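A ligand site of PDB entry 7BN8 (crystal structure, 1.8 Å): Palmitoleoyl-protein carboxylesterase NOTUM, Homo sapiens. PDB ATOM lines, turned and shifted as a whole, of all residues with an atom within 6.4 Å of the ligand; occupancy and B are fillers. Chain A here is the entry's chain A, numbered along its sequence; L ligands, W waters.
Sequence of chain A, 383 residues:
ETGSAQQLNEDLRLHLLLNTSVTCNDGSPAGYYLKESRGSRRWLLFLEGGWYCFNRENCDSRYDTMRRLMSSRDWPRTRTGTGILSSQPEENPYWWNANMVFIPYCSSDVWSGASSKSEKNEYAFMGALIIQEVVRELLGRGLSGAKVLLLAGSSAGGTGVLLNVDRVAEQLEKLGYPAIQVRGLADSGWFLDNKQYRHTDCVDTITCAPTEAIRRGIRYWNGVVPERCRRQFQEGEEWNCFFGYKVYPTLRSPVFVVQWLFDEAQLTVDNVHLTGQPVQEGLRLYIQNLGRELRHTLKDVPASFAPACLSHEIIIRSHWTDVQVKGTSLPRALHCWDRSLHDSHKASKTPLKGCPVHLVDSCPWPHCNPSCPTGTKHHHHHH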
ATOM      1  N   GLY A  49     -11.259  18.062   7.173  1.00  0.00           N
ATOM      2  CA  GLY A  49     -10.315  18.076   6.076  1.00  0.00           C
ATOM      3  C   GLY A  49     -10.835  18.811   4.827  1.00  0.00           C
ATOM      4  O   GLY A  49     -11.809  19.565   4.869  1.00  0.00           O
ATOM      5  N   GLY A  50     -10.137  18.621   3.710  1.00  0.00           N
ATOM      6  CA  GLY A  50     -10.493  19.305   2.454  1.00  0.00           C
ATOM      7  C   GLY A  50      -9.349  19.879   1.622  1.00  0.00           C
ATOM      8  O   GLY A  50      -9.419  21.026   1.164  1.00  0.00           O
ATOM      9  N   TRP A  51      -8.261  19.119   1.447  1.00  0.00           N
ATOM     10  CA  TRP A  51      -7.088  19.543   0.628  1.00  0.00           C
ATOM     11  C   TRP A  51      -6.481  20.842   1.198  1.00  0.00           C
ATOM     12  O   TRP A  51      -6.394  20.984   2.425  1.00  0.00           O
ATOM     13  CB  TRP A  51      -7.515  19.615  -0.834  1.00  0.00           C
ATOM     14  CG  TRP A  51      -7.788  18.223  -1.457  1.00  0.00           C
ATOM     15  CD1 TRP A  51      -9.002  17.631  -1.592  1.00  0.00           C
ATOM     16  CD2 TRP A  51      -6.831  17.279  -1.976  1.00  0.00           C
ATOM     17  NE1 TRP A  51      -8.872  16.394  -2.167  1.00  0.00           N
ATOM     18  CE2 TRP A  51      -7.552  16.149  -2.428  1.00  0.00           C
ATOM     19  CE3 TRP A  51      -5.446  17.290  -2.130  1.00  0.00           C
ATOM     20  CZ2 TRP A  51      -6.940  15.043  -3.007  1.00  0.00           C
ATOM     21  CZ3 TRP A  51      -4.830  16.176  -2.714  1.00  0.00           C
ATOM     22  CH2 TRP A  51      -5.593  15.071  -3.154  1.00  0.00           C
ATOM     23  N   TYR A  52      -6.053  21.791   0.344  1.00  0.00           N
ATOM     24  CA  TYR A  52      -5.267  22.971   0.724  1.00  0.00           C
ATOM     25  C   TYR A  52      -5.017  23.797  -0.534  1.00  0.00           C
ATOM     26  O   TYR A  52      -5.348  23.379  -1.640  1.00  0.00           O
ATOM     27  CB  TYR A  52      -3.935  22.589   1.412  1.00  0.00           C
ATOM     28  CG  TYR A  52      -3.125  21.606   0.581  1.00  0.00           C
ATOM     29  CD1 TYR A  52      -2.370  22.045  -0.493  1.00  0.00           C
ATOM     30  CD2 TYR A  52      -3.176  20.238   0.846  1.00  0.00           C
ATOM     31  CE1 TYR A  52      -1.662  21.132  -1.282  1.00  0.00           C
ATOM     32  CE2 TYR A  52      -2.462  19.330   0.071  1.00  0.00           C
ATOM     33  CZ  TYR A  52      -1.713  19.787  -0.993  1.00  0.00           C
ATOM     34  OH  TYR A  52      -0.996  18.908  -1.774  1.00  0.00           O
ATOM     35  N   TYR A 105     -12.562  23.550   8.955  1.00  0.00           N
ATOM     36  CA  TYR A 105     -11.279  23.802   8.300  1.00  0.00           C
ATOM     37  C   TYR A 105     -11.482  25.025   7.409  1.00  0.00           C
ATOM     38  O   TYR A 105     -12.167  24.935   6.392  1.00  0.00           O
ATOM     39  CB  TYR A 105     -10.891  22.576   7.484  1.00  0.00           C
ATOM     40  CG  TYR A 105      -9.589  22.591   6.703  1.00  0.00           C
ATOM     41  CD1 TYR A 105      -8.405  23.146   7.237  1.00  0.00           C
ATOM     42  CD2 TYR A 105      -9.523  21.962   5.451  1.00  0.00           C
ATOM     43  CE1 TYR A 105      -7.185  23.077   6.508  1.00  0.00           C
ATOM     44  CE2 TYR A 105      -8.323  21.912   4.742  1.00  0.00           C
ATOM     45  CZ  TYR A 105      -7.171  22.467   5.275  1.00  0.00           C
ATOM     46  OH  TYR A 105      -6.006  22.393   4.563  1.00  0.00           O
ATOM     47  N   VAL A 110      -3.359  22.695   5.794  1.00  0.00           N
ATOM     48  CA  VAL A 110      -3.225  21.424   6.518  1.00  0.00           C
ATOM     49  C   VAL A 110      -3.098  21.649   8.054  1.00  0.00           C
ATOM     50  O   VAL A 110      -2.440  20.869   8.752  1.00  0.00           O
ATOM     51  CB  VAL A 110      -2.056  20.581   5.963  1.00  0.00           C
ATOM     52  CG1 VAL A 110      -2.191  19.103   6.380  1.00  0.00           C
ATOM     53  CG2 VAL A 110      -2.011  20.651   4.425  1.00  0.00           C
ATOM     54  N   SER A 154      -9.966  13.896   9.878  1.00  0.00           N
ATOM     55  CA  SER A 154     -10.000  13.128   8.637  1.00  0.00           C
ATOM     56  C   SER A 154      -9.323  13.893   7.495  1.00  0.00           C
ATOM     57  O   SER A 154      -9.465  15.120   7.382  1.00  0.00           O
ATOM     58  CB  SER A 154     -11.463  12.798   8.219  1.00  0.00           C
ATOM     59  OG  SER A 154     -12.116  11.972   9.171  1.00  0.00           O
ATOM     60  N   SER A 155      -8.622  13.168   6.636  1.00  0.00           N
ATOM     61  CA  SER A 155      -7.968  13.740   5.412  1.00  0.00           C
ATOM     62  C   SER A 155      -6.932  14.764   5.870  1.00  0.00           C
ATOM     63  O   SER A 155      -6.039  14.426   6.671  1.00  0.00           O
ATOM     64  CB  SER A 155      -8.988  14.323   4.428  1.00  0.00           C
ATOM     65  OG  SER A 155      -9.913  13.377   3.995  1.00  0.00           O
ATOM     66  N   ALA A 156      -6.993  16.010   5.386  1.00  0.00           N
ATOM     67  CA  ALA A 156      -6.065  17.032   5.860  1.00  0.00           C
ATOM     68  C   ALA A 156      -6.165  17.225   7.354  1.00  0.00           C
ATOM     69  O   ALA A 156      -5.181  17.628   7.988  1.00  0.00           O
ATOM     70  CB  ALA A 156      -6.326  18.392   5.165  1.00  0.00           C
ATOM     71  N   GLY A 157      -7.359  16.979   7.927  1.00  0.00           N
ATOM     72  CA  GLY A 157      -7.491  17.010   9.390  1.00  0.00           C
ATOM     73  C   GLY A 157      -6.762  15.892  10.105  1.00  0.00           C
ATOM     74  O   GLY A 157      -6.349  16.051  11.269  1.00  0.00           O
ATOM     75  N   THR A 159      -3.860  14.569   8.948  1.00  0.00           N
ATOM     76  CA  THR A 159      -2.475  15.037   8.992  1.00  0.00           C
ATOM     77  C   THR A 159      -2.327  16.128  10.061  1.00  0.00           C
ATOM     78  O   THR A 159      -1.314  16.177  10.780  1.00  0.00           O
ATOM     79  CB  THR A 159      -2.051  15.571   7.599  1.00  0.00           C
ATOM     80  OG1 THR A 159      -2.392  14.585   6.598  1.00  0.00           O
ATOM     81  CG2 THR A 159      -0.550  15.852   7.539  1.00  0.00           C
ATOM     82  N   SER A 188      -7.178   8.759   7.562  1.00  0.00           N
ATOM     83  CA  SER A 188      -6.938   9.074   6.132  1.00  0.00           C
ATOM     84  C   SER A 188      -5.967  10.237   5.945  1.00  0.00           C
ATOM     85  O   SER A 188      -6.031  10.977   4.941  1.00  0.00           O
ATOM     86  CB  SER A 188      -8.226   9.399   5.358  1.00  0.00           C
ATOM     87  OG  SER A 188      -9.068   8.260   5.247  1.00  0.00           O
ATOM     88  N   GLY A 189      -5.032  10.409   6.874  1.00  0.00           N
ATOM     89  CA  GLY A 189      -4.021  11.434   6.684  1.00  0.00           C
ATOM     90  C   GLY A 189      -2.579  10.956   6.669  1.00  0.00           C
ATOM     91  O   GLY A 189      -1.647  11.754   6.909  1.00  0.00           O
ATOM     92  N   PHE A 191       0.085   9.570   4.341  1.00  0.00           N
ATOM     93  CA  PHE A 191       0.445   9.520   2.927  1.00  0.00           C
ATOM     94  C   PHE A 191       1.897   9.140   2.726  1.00  0.00           C
ATOM     95  O   PHE A 191       2.729   9.288   3.624  1.00  0.00           O
ATOM     96  CB  PHE A 191       0.161  10.869   2.258  1.00  0.00           C
ATOM     97  CG  PHE A 191      -1.276  11.247   2.334  1.00  0.00           C
ATOM     98  CD1 PHE A 191      -2.197  10.564   1.576  1.00  0.00           C
ATOM     99  CD2 PHE A 191      -1.722  12.203   3.240  1.00  0.00           C
ATOM    100  CE1 PHE A 191      -3.563  10.860   1.680  1.00  0.00           C
ATOM    101  CE2 PHE A 191      -3.081  12.519   3.332  1.00  0.00           C
ATOM    102  CZ  PHE A 191      -4.005  11.854   2.561  1.00  0.00           C
ATOM    103  N   LEU A 192       2.192   8.655   1.507  1.00  0.00           N
ATOM    104  CA  LEU A 192       3.524   8.290   1.047  1.00  0.00           C
ATOM    105  C   LEU A 192       4.029   9.296   0.001  1.00  0.00           C
ATOM    106  O   LEU A 192       3.271   9.713  -0.898  1.00  0.00           O
ATOM    107  CB  LEU A 192       3.533   6.885   0.409  1.00  0.00           C
ATOM    108  CG  LEU A 192       2.987   5.736   1.286  1.00  0.00           C
ATOM    109  CD1 LEU A 192       3.008   4.402   0.494  1.00  0.00           C
ATOM    110  CD2 LEU A 192       3.751   5.665   2.653  1.00  0.00           C
ATOM    111  N   PRO A 210       2.753  14.885  -4.213  1.00  0.00           N
ATOM    112  CA  PRO A 210       2.588  15.399  -2.835  1.00  0.00           C
ATOM    113  C   PRO A 210       3.793  16.205  -2.336  1.00  0.00           C
ATOM    114  O   PRO A 210       3.620  17.291  -1.754  1.00  0.00           O
ATOM    115  CB  PRO A 210       2.331  14.131  -2.018  1.00  0.00           C
ATOM    116  CG  PRO A 210       2.770  12.950  -2.885  1.00  0.00           C
ATOM    117  CD  PRO A 210       2.606  13.417  -4.314  1.00  0.00           C
ATOM    118  N   THR A 211       5.014  15.737  -2.631  1.00  0.00           N
ATOM    119  CA  THR A 211       6.222  16.373  -2.121  1.00  0.00           C
ATOM    120  C   THR A 211       6.322  17.851  -2.517  1.00  0.00           C
ATOM    121  O   THR A 211       6.570  18.713  -1.667  1.00  0.00           O
ATOM    122  CB  THR A 211       7.438  15.599  -2.636  1.00  0.00           C
ATOM    123  OG1 THR A 211       7.498  14.326  -1.962  1.00  0.00           O
ATOM    124  CG2 THR A 211       8.669  16.332  -2.367  1.00  0.00           C
ATOM    125  N   ILE A 214       3.582  20.413  -0.916  1.00  0.00           N
ATOM    126  CA  ILE A 214       3.837  20.729   0.494  1.00  0.00           C
ATOM    127  C   ILE A 214       5.029  21.682   0.651  1.00  0.00           C
ATOM    128  O   ILE A 214       5.003  22.588   1.485  1.00  0.00           O
ATOM    129  CB  ILE A 214       4.042  19.442   1.304  1.00  0.00           C
ATOM    130  CG1 ILE A 214       2.811  18.520   1.242  1.00  0.00           C
ATOM    131  CG2 ILE A 214       4.421  19.769   2.761  1.00  0.00           C
ATOM    132  CD1 ILE A 214       1.561  19.140   1.775  1.00  0.00           C
ATOM    133  N   PHE A 242       5.212  16.435   7.267  1.00  0.00           N
ATOM    134  CA  PHE A 242       3.835  16.268   6.828  1.00  0.00           C
ATOM    135  C   PHE A 242       3.529  14.836   6.420  1.00  0.00           C
ATOM    136  O   PHE A 242       2.368  14.554   6.067  1.00  0.00           O
ATOM    137  CB  PHE A 242       3.514  17.194   5.636  1.00  0.00           C
ATOM    138  CG  PHE A 242       3.269  18.629   6.038  1.00  0.00           C
ATOM    139  CD1 PHE A 242       4.305  19.384   6.556  1.00  0.00           C
ATOM    140  CD2 PHE A 242       2.027  19.236   5.838  1.00  0.00           C
ATOM    141  CE1 PHE A 242       4.108  20.716   6.917  1.00  0.00           C
ATOM    142  CE2 PHE A 242       1.819  20.583   6.183  1.00  0.00           C
ATOM    143  CZ  PHE A 242       2.855  21.306   6.741  1.00  0.00           C
ATOM    144  N   PHE A 243       4.515  13.933   6.470  1.00  0.00           N
ATOM    145  CA  PHE A 243       4.349  12.568   6.014  1.00  0.00           C
ATOM    146  C   PHE A 243       4.356  11.651   7.228  1.00  0.00           C
ATOM    147  O   PHE A 243       5.355  11.566   7.942  1.00  0.00           O
ATOM    148  CB  PHE A 243       5.427  12.211   4.976  1.00  0.00           C
ATOM    149  CG  PHE A 243       5.157  12.877   3.636  1.00  0.00           C
ATOM    150  CD1 PHE A 243       5.627  14.144   3.376  1.00  0.00           C
ATOM    151  CD2 PHE A 243       4.308  12.278   2.723  1.00  0.00           C
ATOM    152  CE1 PHE A 243       5.315  14.780   2.177  1.00  0.00           C
ATOM    153  CE2 PHE A 243       3.982  12.915   1.535  1.00  0.00           C
ATOM    154  CZ  PHE A 243       4.461  14.152   1.270  1.00  0.00           C
ATOM    155  N   ASP A 263      -5.896   4.433  -0.446  1.00  0.00           N
ATOM    156  CA  ASP A 263      -6.607   5.698  -0.275  1.00  0.00           C
ATOM    157  C   ASP A 263      -6.804   6.431  -1.598  1.00  0.00           C
ATOM    158  O   ASP A 263      -5.864   6.599  -2.374  1.00  0.00           O
ATOM    159  CB  ASP A 263      -5.813   6.570   0.690  1.00  0.00           C
ATOM    160  CG  ASP A 263      -6.571   7.787   1.105  1.00  0.00           C
ATOM    161  OD1 ASP A 263      -7.287   7.730   2.135  1.00  0.00           O
ATOM    162  OD2 ASP A 263      -6.456   8.803   0.394  1.00  0.00           O
ATOM    163  N   ALA A 265      -7.268   9.537  -2.257  1.00  0.00           N
ATOM    164  CA  ALA A 265      -6.491  10.762  -2.410  1.00  0.00           C
ATOM    165  C   ALA A 265      -5.033  10.443  -2.725  1.00  0.00           C
ATOM    166  O   ALA A 265      -4.390  11.165  -3.483  1.00  0.00           O
ATOM    167  CB  ALA A 265      -6.592  11.622  -1.150  1.00  0.00           C
ATOM    168  N   GLN A 266      -4.482   9.391  -2.110  1.00  0.00           N
ATOM    169  CA  GLN A 266      -3.155   8.886  -2.509  1.00  0.00           C
ATOM    170  C   GLN A 266      -3.112   8.505  -3.982  1.00  0.00           C
ATOM    171  O   GLN A 266      -2.152   8.814  -4.693  1.00  0.00           O
ATOM    172  CB  GLN A 266      -2.801   7.650  -1.662  1.00  0.00           C
ATOM    173  CG  GLN A 266      -1.401   7.042  -1.965  1.00  0.00           C
ATOM    174  CD  GLN A 266      -0.268   7.866  -1.347  1.00  0.00           C
ATOM    175  OE1 GLN A 266      -0.248   8.114  -0.146  1.00  0.00           O
ATOM    176  NE2 GLN A 266       0.718   8.247  -2.177  1.00  0.00           N
ATOM    177  N   VAL A 269      -3.140  11.840  -6.242  1.00  0.00           N
ATOM    178  CA  VAL A 269      -1.824  12.482  -6.358  1.00  0.00           C
ATOM    179  C   VAL A 269      -0.839  11.610  -7.110  1.00  0.00           C
ATOM    180  O   VAL A 269       0.105  12.144  -7.691  1.00  0.00           O
ATOM    181  CB  VAL A 269      -1.238  12.882  -4.976  1.00  0.00           C
ATOM    182  CG1 VAL A 269      -2.186  13.797  -4.256  1.00  0.00           C
ATOM    183  CG2 VAL A 269      -0.852  11.683  -4.085  1.00  0.00           C
ATOM    184  N   HIS A 312     -12.021   6.704   1.012  1.00  0.00           N
ATOM    185  CA  HIS A 312     -11.414   7.938   1.570  1.00  0.00           C
ATOM    186  C   HIS A 312     -12.231   8.407   2.774  1.00  0.00           C
ATOM    187  O   HIS A 312     -13.424   8.647   2.630  1.00  0.00           O
ATOM    188  CB  HIS A 312     -11.362   9.035   0.490  1.00  0.00           C
ATOM    189  CG  HIS A 312     -10.555  10.245   0.876  1.00  0.00           C
ATOM    190  ND1 HIS A 312      -9.232  10.159   1.257  1.00  0.00           N
ATOM    191  CD2 HIS A 312     -10.885  11.560   0.936  1.00  0.00           C
ATOM    192  CE1 HIS A 312      -8.787  11.373   1.546  1.00  0.00           C
ATOM    193  NE2 HIS A 312      -9.773  12.233   1.348  1.00  0.00           N
ATOM    194  N   GLU A 313     -11.567   8.579   3.937  1.00  0.00           N
ATOM    195  CA  GLU A 313     -12.187   8.923   5.232  1.00  0.00           C
ATOM    196  C   GLU A 313     -13.152   7.853   5.775  1.00  0.00           C
ATOM    197  O   GLU A 313     -13.649   7.011   5.024  1.00  0.00           O
ATOM    198  CB  GLU A 313     -12.959  10.253   5.207  1.00  0.00           C
ATOM    199  CG  GLU A 313     -12.138  11.445   4.733  1.00  0.00           C
ATOM    200  CD  GLU A 313     -12.946  12.751   4.704  1.00  0.00           C
ATOM    201  OE1 GLU A 313     -14.199  12.691   4.544  1.00  0.00           O
ATOM    202  OE2 GLU A 313     -12.333  13.830   4.827  1.00  0.00           O
HETATM  203  C1  LIG L   1      -1.305  15.735   3.369  1.00  0.00           C
HETATM  204  C2  LIG L   1       0.994  15.241   2.712  1.00  0.00           C
HETATM  205  C3  LIG L   1      -0.812  15.027   1.088  1.00  0.00           C
HETATM  206  C4  LIG L   1      -1.323  14.686  -0.327  1.00  0.00           C
HETATM  207  C5  LIG L   1      -2.691  14.107  -0.350  1.00  0.00           C
HETATM  208  C6  LIG L   1      -3.663  14.818   0.611  1.00  0.00           C
HETATM  209  C7  LIG L   1      -5.099  14.902   0.518  1.00  0.00           C
HETATM  210  C8  LIG L   1      -5.757  15.623   1.536  1.00  0.00           C
HETATM  211  C9  LIG L   1      -7.280  15.856   1.666  1.00  0.00           C
HETATM  212  C10 LIG L   1      -3.156  15.499   1.731  1.00  0.00           C
HETATM  213  C11 LIG L   1      -1.728  15.461   2.052  1.00  0.00           C
HETATM  214  C12 LIG L   1       0.056  15.641   3.679  1.00  0.00           C
HETATM  215  C13 LIG L   1       0.545  14.936   1.412  1.00  0.00           C
HETATM  216  O1  LIG L   1      -7.857  16.631   2.524  1.00  0.00           O
HETATM  217  O2  LIG L   1      -8.005  15.154   0.909  1.00  0.00           O
HETATM  218  S1  LIG L   1      -4.494  16.162   2.532  1.00  0.00           S
HETATM  219  O   HOH W   1     -10.604  15.582   1.514  1.00  0.00           O
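O1 of the ligand is in hydrogen-bond range of N of Trp 51 (2.7 Å). The indole nitrogen (NE1) of Trp 51 is in hydrogen-bond range of an oxygen (O2) of the ligand (3.4 Å). The backbone NH (N) of Ala 156 lies within hydrogen-bond range of an oxygen (O1) of the ligand (3.1 Å). The backbone NH (N) of Gly 50 lies within hydrogen-bond range of an oxygen (O1) of the ligand (3.3 Å). O2 of the ligand sits at hydrogen-bond distance from NE2 of His 312, at 3.4 Å.
Water W1 lies within hydrogen-bond range of O2 of the ligand, OG of Ser 155 and NE2 of His 312.
The backbone carbonyl oxygen (O) of Trp 51 lies within hydrogen-bond range of the side-chain hydroxyl (OH) of Tyr 105 (2.6 Å). The side-chain hydroxyl (OG) of Ser 155 sits at hydrogen-bond distance from a ring nitrogen (NE2) of His 312 (2.9 Å). The side-chain hydroxyl (OG) of Ser 155 sits at hydrogen-bond distance from the side-chain carboxylate (OE2) of Glu 313. A ring nitrogen (ND1) of His 312 sits at hydrogen-bond distance from the side-chain carboxylate (OD2) of Asp 263 (3.2 Å). The side-chain hydroxyl (OG1) of Thr 159 lies within hydrogen-bond range of the backbone carbonyl oxygen (O) of Gly 189 (2.9 Å). The backbone NH of Ala 265 lies within hydrogen-bond range of the side-chain carboxylate of Asp 263 (2.9 Å).
Ser 155 touches the ligand. OG1 of Thr 159 touches C1 of the ligand, 3.6 Å away. Phe 191 touches the ligand. CB of Pro 210 touches C13 of the ligand (3.95 Å). Phe 242 touches the ligand (O to C12, 3.5 Å). Phe 243 touches the ligand. Ala 265 touches the ligand. Val 269 touches the ligand (CG1 to C5, 3.95 Å). Hydrophobic or aromatic side chains that line the ligand: Trp 51, Ala 156, Phe 191, Pro 210, Phe 243, Ala 265, Val 269 and His 312. Of the 26 residues printed, 12 come within 4 Å of the ligand. Along chain A the residues within 4 Å of the ligand span positions 50 to 312.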
